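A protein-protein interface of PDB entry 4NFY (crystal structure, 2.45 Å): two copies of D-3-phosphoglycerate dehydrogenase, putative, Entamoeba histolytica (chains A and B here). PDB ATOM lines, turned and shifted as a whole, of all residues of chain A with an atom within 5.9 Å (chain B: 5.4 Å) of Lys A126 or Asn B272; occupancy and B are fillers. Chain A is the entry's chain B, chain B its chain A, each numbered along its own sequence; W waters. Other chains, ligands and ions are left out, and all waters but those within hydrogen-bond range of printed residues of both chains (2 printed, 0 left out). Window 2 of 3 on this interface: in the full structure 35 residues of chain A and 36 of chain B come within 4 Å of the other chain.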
ATOM      1  N   PHE A 118      16.918  13.563   1.130  1.00  0.00           N
ATOM      2  CA  PHE A 118      17.771  14.423   1.980  1.00  0.00           C
ATOM      3  C   PHE A 118      17.073  14.932   3.236  1.00  0.00           C
ATOM      4  O   PHE A 118      17.754  15.362   4.177  1.00  0.00           O
ATOM      5  CB  PHE A 118      18.338  15.622   1.195  1.00  0.00           C
ATOM      6  CG  PHE A 118      19.793  15.490   0.791  1.00  0.00           C
ATOM      7  CD1 PHE A 118      20.466  14.257   0.804  1.00  0.00           C
ATOM      8  CD2 PHE A 118      20.493  16.619   0.358  1.00  0.00           C
ATOM      9  CE1 PHE A 118      21.796  14.170   0.423  1.00  0.00           C
ATOM     10  CE2 PHE A 118      21.821  16.528  -0.029  1.00  0.00           C
ATOM     11  CZ  PHE A 118      22.470  15.300   0.003  1.00  0.00           C
ATOM     12  N   LYS A 120      14.763  13.053   5.062  1.00  0.00           N
ATOM     13  CA  LYS A 120      14.289  11.923   5.846  1.00  0.00           C
ATOM     14  C   LYS A 120      12.848  11.564   5.581  1.00  0.00           C
ATOM     15  O   LYS A 120      12.112  11.183   6.492  1.00  0.00           O
ATOM     16  CB  LYS A 120      14.502  12.194   7.338  1.00  0.00           C
ATOM     17  CG  LYS A 120      15.965  12.189   7.758  1.00  0.00           C
ATOM     18  CD  LYS A 120      16.112  11.795   9.225  1.00  0.00           C
ATOM     19  CE  LYS A 120      17.423  11.071   9.519  1.00  0.00           C
ATOM     20  NZ  LYS A 120      18.605  11.797   8.966  1.00  0.00           N
ATOM     21  N   GLU A 124      11.014  13.521  11.145  1.00  0.00           N
ATOM     22  CA  GLU A 124      11.914  14.162  12.087  1.00  0.00           C
ATOM     23  C   GLU A 124      13.349  13.693  11.857  1.00  0.00           C
ATOM     24  O   GLU A 124      13.576  12.539  11.507  1.00  0.00           O
ATOM     25  CB  GLU A 124      11.456  13.846  13.517  1.00  0.00           C
ATOM     26  CG  GLU A 124      12.133  14.668  14.603  1.00  0.00           C
ATOM     27  CD  GLU A 124      11.453  14.525  15.959  1.00  0.00           C
ATOM     28  OE1 GLU A 124      10.273  14.100  16.012  1.00  0.00           O
ATOM     29  OE2 GLU A 124      12.099  14.851  16.977  1.00  0.00           O
ATOM     30  N   GLY A 125      14.297  14.609  12.037  1.00  0.00           N
ATOM     31  CA  GLY A 125      15.726  14.299  11.957  1.00  0.00           C
ATOM     32  C   GLY A 125      16.539  15.339  11.194  1.00  0.00           C
ATOM     33  O   GLY A 125      16.007  16.312  10.682  1.00  0.00           O
ATOM     34  N   LYS A 126      17.841  15.104  11.110  1.00  0.00           N
ATOM     35  CA  LYS A 126      18.773  16.084  10.581  1.00  0.00           C
ATOM     36  C   LYS A 126      18.832  15.995   9.059  1.00  0.00           C
ATOM     37  O   LYS A 126      19.344  15.023   8.513  1.00  0.00           O
ATOM     38  CB  LYS A 126      20.174  15.866  11.178  1.00  0.00           C
ATOM     39  CG  LYS A 126      20.831  17.143  11.687  1.00  0.00           C
ATOM     40  CD  LYS A 126      20.351  17.477  13.099  1.00  0.00           C
ATOM     41  CE  LYS A 126      20.316  18.976  13.354  1.00  0.00           C
ATOM     42  NZ  LYS A 126      19.236  19.664  12.581  1.00  0.00           N
ATOM     43  N   GLY A 127      18.315  17.012   8.381  1.00  0.00           N
ATOM     44  CA  GLY A 127      18.286  17.035   6.919  1.00  0.00           C
ATOM     45  C   GLY A 127      19.531  17.639   6.293  1.00  0.00           C
ATOM     46  O   GLY A 127      20.413  18.126   6.986  1.00  0.00           O
ATOM     47  N   ARG A 128      19.586  17.593   4.969  1.00  0.00           N
ATOM     48  CA  ARG A 128      20.625  18.238   4.186  1.00  0.00           C
ATOM     49  C   ARG A 128      19.983  18.968   3.009  1.00  0.00           C
ATOM     50  O   ARG A 128      18.793  18.794   2.744  1.00  0.00           O
ATOM     51  CB  ARG A 128      21.630  17.207   3.687  1.00  0.00           C
ATOM     52  CG  ARG A 128      22.425  16.529   4.794  1.00  0.00           C
ATOM     53  CD  ARG A 128      23.612  15.757   4.233  1.00  0.00           C
ATOM     54  NE  ARG A 128      24.232  14.881   5.235  1.00  0.00           N
ATOM     55  CZ  ARG A 128      25.503  14.953   5.671  1.00  0.00           C
ATOM     56  NH1 ARG A 128      26.364  15.862   5.206  1.00  0.00           N
ATOM     57  NH2 ARG A 128      25.926  14.093   6.594  1.00  0.00           N
ATOM     58  N   PHE B  11      27.221  22.184  18.244  1.00  0.00           N
ATOM     59  CA  PHE B  11      27.276  22.359  16.806  1.00  0.00           C
ATOM     60  C   PHE B  11      28.052  21.190  16.229  1.00  0.00           C
ATOM     61  O   PHE B  11      28.805  20.530  16.931  1.00  0.00           O
ATOM     62  CB  PHE B  11      28.044  23.623  16.434  1.00  0.00           C
ATOM     63  CG  PHE B  11      27.299  24.906  16.655  1.00  0.00           C
ATOM     64  CD1 PHE B  11      26.321  25.316  15.767  1.00  0.00           C
ATOM     65  CD2 PHE B  11      27.639  25.752  17.709  1.00  0.00           C
ATOM     66  CE1 PHE B  11      25.670  26.522  15.942  1.00  0.00           C
ATOM     67  CE2 PHE B  11      26.985  26.958  17.889  1.00  0.00           C
ATOM     68  CZ  PHE B  11      26.002  27.344  17.001  1.00  0.00           C
ATOM     69  N   ALA B  15      31.329  23.249  12.046  1.00  0.00           N
ATOM     70  CA  ALA B  15      30.742  24.523  12.466  1.00  0.00           C
ATOM     71  C   ALA B  15      31.584  25.126  13.577  1.00  0.00           C
ATOM     72  O   ALA B  15      31.922  26.309  13.543  1.00  0.00           O
ATOM     73  CB  ALA B  15      29.300  24.336  12.924  1.00  0.00           C
ATOM     74  N   ARG B  55      22.622  28.368  21.296  1.00  0.00           N
ATOM     75  CA  ARG B  55      21.621  27.786  20.425  1.00  0.00           C
ATOM     76  C   ARG B  55      20.326  28.010  21.183  1.00  0.00           C
ATOM     77  O   ARG B  55      20.092  29.120  21.652  1.00  0.00           O
ATOM     78  CB  ARG B  55      21.942  26.317  20.190  1.00  0.00           C
ATOM     79  CG  ARG B  55      23.356  26.084  19.676  1.00  0.00           C
ATOM     80  CD  ARG B  55      23.401  25.605  18.237  1.00  0.00           C
ATOM     81  NE  ARG B  55      23.527  24.154  18.180  1.00  0.00           N
ATOM     82  CZ  ARG B  55      22.795  23.327  17.437  1.00  0.00           C
ATOM     83  NH1 ARG B  55      21.854  23.770  16.615  1.00  0.00           N
ATOM     84  NH2 ARG B  55      23.040  22.026  17.510  1.00  0.00           N
ATOM     85  N   ALA B 266      13.841  24.256   8.988  1.00  0.00           N
ATOM     86  CA  ALA B 266      15.139  24.784   9.404  1.00  0.00           C
ATOM     87  C   ALA B 266      16.085  23.708   9.906  1.00  0.00           C
ATOM     88  O   ALA B 266      17.234  24.010  10.250  1.00  0.00           O
ATOM     89  CB  ALA B 266      14.938  25.830  10.498  1.00  0.00           C
ATOM     90  N   GLU B 267      15.613  22.465   9.950  1.00  0.00           N
ATOM     91  CA  GLU B 267      16.413  21.339  10.442  1.00  0.00           C
ATOM     92  C   GLU B 267      17.358  20.795   9.385  1.00  0.00           C
ATOM     93  O   GLU B 267      17.174  19.677   8.907  1.00  0.00           O
ATOM     94  CB  GLU B 267      15.501  20.198  10.895  1.00  0.00           C
ATOM     95  CG  GLU B 267      14.768  20.480  12.175  1.00  0.00           C
ATOM     96  CD  GLU B 267      15.722  20.538  13.351  1.00  0.00           C
ATOM     97  OE1 GLU B 267      16.418  19.523  13.624  1.00  0.00           O
ATOM     98  OE2 GLU B 267      15.770  21.607  13.987  1.00  0.00           O
ATOM     99  N   THR B 268      18.376  21.562   9.024  1.00  0.00           N
ATOM    100  CA  THR B 268      19.383  21.059   8.090  1.00  0.00           C
ATOM    101  C   THR B 268      20.751  21.382   8.625  1.00  0.00           C
ATOM    102  O   THR B 268      20.937  22.401   9.265  1.00  0.00           O
ATOM    103  CB  THR B 268      19.259  21.652   6.666  1.00  0.00           C
ATOM    104  OG1 THR B 268      19.547  23.053   6.688  1.00  0.00           O
ATOM    105  CG2 THR B 268      17.871  21.418   6.114  1.00  0.00           C
ATOM    106  N   GLU B 269      21.713  20.512   8.345  1.00  0.00           N
ATOM    107  CA  GLU B 269      23.078  20.730   8.813  1.00  0.00           C
ATOM    108  C   GLU B 269      23.602  22.090   8.354  1.00  0.00           C
ATOM    109  O   GLU B 269      24.286  22.796   9.105  1.00  0.00           O
ATOM    110  CB  GLU B 269      23.980  19.606   8.331  1.00  0.00           C
ATOM    111  CG  GLU B 269      23.698  18.299   9.045  1.00  0.00           C
ATOM    112  CD  GLU B 269      24.287  17.106   8.329  1.00  0.00           C
ATOM    113  OE1 GLU B 269      25.161  17.311   7.440  1.00  0.00           O
ATOM    114  OE2 GLU B 269      23.861  15.970   8.651  1.00  0.00           O
ATOM    115  N   GLU B 270      23.231  22.461   7.135  1.00  0.00           N
ATOM    116  CA  GLU B 270      23.626  23.733   6.571  1.00  0.00           C
ATOM    117  C   GLU B 270      23.017  24.891   7.351  1.00  0.00           C
ATOM    118  O   GLU B 270      23.712  25.851   7.661  1.00  0.00           O
ATOM    119  CB  GLU B 270      23.228  23.813   5.096  1.00  0.00           C
ATOM    120  CG  GLU B 270      23.912  22.779   4.207  1.00  0.00           C
ATOM    121  CD  GLU B 270      23.153  21.459   4.129  1.00  0.00           C
ATOM    122  OE1 GLU B 270      22.251  21.239   4.971  1.00  0.00           O
ATOM    123  OE2 GLU B 270      23.448  20.651   3.217  1.00  0.00           O
ATOM    124  N   SER B 271      21.727  24.801   7.678  1.00  0.00           N
ATOM    125  CA  SER B 271      21.089  25.834   8.494  1.00  0.00           C
ATOM    126  C   SER B 271      21.855  26.064   9.798  1.00  0.00           C
ATOM    127  O   SER B 271      22.107  27.200  10.178  1.00  0.00           O
ATOM    128  CB  SER B 271      19.626  25.487   8.796  1.00  0.00           C
ATOM    129  OG  SER B 271      18.844  25.567   7.615  1.00  0.00           O
ATOM    130  N   ASN B 272      22.237  24.982  10.463  1.00  0.00           N
ATOM    131  CA  ASN B 272      22.961  25.068  11.739  1.00  0.00           C
ATOM    132  C   ASN B 272      24.370  25.629  11.657  1.00  0.00           C
ATOM    133  O   ASN B 272      24.771  26.392  12.534  1.00  0.00           O
ATOM    134  CB  ASN B 272      22.980  23.712  12.440  1.00  0.00           C
ATOM    135  CG  ASN B 272      21.596  23.253  12.826  1.00  0.00           C
ATOM    136  OD1 ASN B 272      20.693  24.072  13.039  1.00  0.00           O
ATOM    137  ND2 ASN B 272      21.413  21.943  12.915  1.00  0.00           N
ATOM    138  N   ILE B 273      25.122  25.276  10.626  1.00  0.00           N
ATOM    139  CA  ILE B 273      26.467  25.872  10.461  1.00  0.00           C
ATOM    140  C   ILE B 273      26.359  27.320   9.975  1.00  0.00           C
ATOM    141  O   ILE B 273      27.133  28.173  10.409  1.00  0.00           O
ATOM    142  CB  ILE B 273      27.429  25.033   9.565  1.00  0.00           C
ATOM    143  CG1 ILE B 273      28.839  25.631   9.586  1.00  0.00           C
ATOM    144  CG2 ILE B 273      26.954  24.952   8.123  1.00  0.00           C
ATOM    145  CD1 ILE B 273      29.822  24.923   8.675  1.00  0.00           C
ATOM    146  N   ASN B 274      25.383  27.608   9.119  1.00  0.00           N
ATOM    147  CA  ASN B 274      25.162  28.992   8.683  1.00  0.00           C
ATOM    148  C   ASN B 274      24.895  29.909   9.862  1.00  0.00           C
ATOM    149  O   ASN B 274      25.430  31.023   9.924  1.00  0.00           O
ATOM    150  CB  ASN B 274      23.975  29.094   7.737  1.00  0.00           C
ATOM    151  CG  ASN B 274      24.219  28.418   6.415  1.00  0.00           C
ATOM    152  OD1 ASN B 274      25.333  27.986   6.107  1.00  0.00           O
ATOM    153  ND2 ASN B 274      23.164  28.298   5.626  1.00  0.00           N
ATOM    154  N   ALA B 275      24.066  29.430  10.790  1.00  0.00           N
ATOM    155  CA  ALA B 275      23.684  30.202  11.965  1.00  0.00           C
ATOM    156  C   ALA B 275      24.856  30.361  12.947  1.00  0.00           C
ATOM    157  O   ALA B 275      25.169  31.464  13.368  1.00  0.00           O
ATOM    158  CB  ALA B 275      22.482  29.564  12.648  1.00  0.00           C
ATOM    159  N   GLY B 276      25.502  29.261  13.301  1.00  0.00           N
ATOM    160  CA  GLY B 276      26.676  29.314  14.162  1.00  0.00           C
ATOM    161  C   GLY B 276      27.765  30.237  13.631  1.00  0.00           C
ATOM    162  O   GLY B 276      28.355  31.018  14.384  1.00  0.00           O
ATOM    163  N   MET B 277      28.043  30.162  12.337  1.00  0.00           N
ATOM    164  CA  MET B 277      29.096  30.994  11.772  1.00  0.00           C
ATOM    165  C   MET B 277      28.660  32.447  11.605  1.00  0.00           C
ATOM    166  O   MET B 277      29.475  33.352  11.735  1.00  0.00           O
ATOM    167  CB  MET B 277      29.634  30.400  10.465  1.00  0.00           C
ATOM    168  CG  MET B 277      30.586  29.235  10.727  1.00  0.00           C
ATOM    169  SD  MET B 277      31.215  28.398   9.262  1.00  0.00           S
ATOM    170  CE  MET B 277      32.094  29.724   8.438  1.00  0.00           C
HETATM  171  O   HOH W   1      15.099  18.109   7.613  1.00  0.00           O
HETATM  172  O   HOH W   2      25.206  18.790   4.111  1.00  0.00           O
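The side-chain carboxylate (OE1) of Glu B267 lies within salt-bridge range of the side-chain amino group (NZ) of Lys A126 (3.0 Å).
O of Glu B267 lies within hydrogen-bond range of N of Gly A127, at 2.9 Å.
O of Gly A127 is in hydrogen-bond range of N of Glu B269 (3.0 Å).
NH1 of Arg A128 is in salt-bridge range of OE1 of Glu B269, at 2.9 Å.
The side-chain amide nitrogen (ND2) of Asn B272 lies close to the side-chain amino group (NZ) of Lys A126, at 3.2 Å.
The side-chain hydroxyl (OG1) of Thr B268 is in hydrogen-bond range of the side-chain hydroxyl (OG) of Ser B271 (2.8 Å).
The side-chain amide oxygen (OD1) of Asn B274 lies close to the backbone carbonyl oxygen (O) of Glu B270 (3.1 Å).
The backbone carbonyl oxygen (O) of Phe A118 is in hydrogen-bond range of the backbone NH (N) of Arg A128 (3.0 Å).
NZ of Lys A120 sits at hydrogen-bond distance from O of Lys A126, at 3.3 Å.
Glu B267 touches Gly A125.
Thr B268 touches Gly A127.
Arg A128 touches Glu B270.
Of chain B, only Glu B267 (3.0 Å) and Asn B272 (3.2 Å) come within 4 Å of Lys A126.
Of chain A, only Lys A126 comes within 4 Å of Asn B272.
Printed residues of chain A within 4 Å of Glu B269: Gly A127 (3.0 Å) and Arg A128 (2.9 Å).
Of the printed residues of chain B, Arg A128 touches Glu B269 and Glu B270.
Of the printed residues of chain B, Gly A125 touches Glu B267.
Of the printed residues of chain B, Gly A127 touches Glu B267 (2.9 Å), Thr B268 (3.3 Å) and Glu B269 (3.0 Å).
Of the printed residues of chain A, Glu B267 touches Gly A125, Lys A126 and Gly A127.
Of the 15 printed residues of chain B, 5 touch a printed residue of chain A.
Printed residues of chain B that touch a printed residue of chain A: Glu B267, Thr B268, Glu B269, Glu B270 and Asn B272.
Of the 7 printed residues of chain A, 4 touch a printed residue of chain B.
Among the printed residues, 8 pairs touch across the chains.
No position is printed for both chains.
Of the 8 pairs that touch across the chains among the printed residues, none has its exchanged pair printed and touching as well.
Water W2 bridges OE2 of Glu B270 (2.7 Å) and NH1 of Arg A128 (3.3 Å).
Water W1 bridges O of Glu B267 and N of Gly A127.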
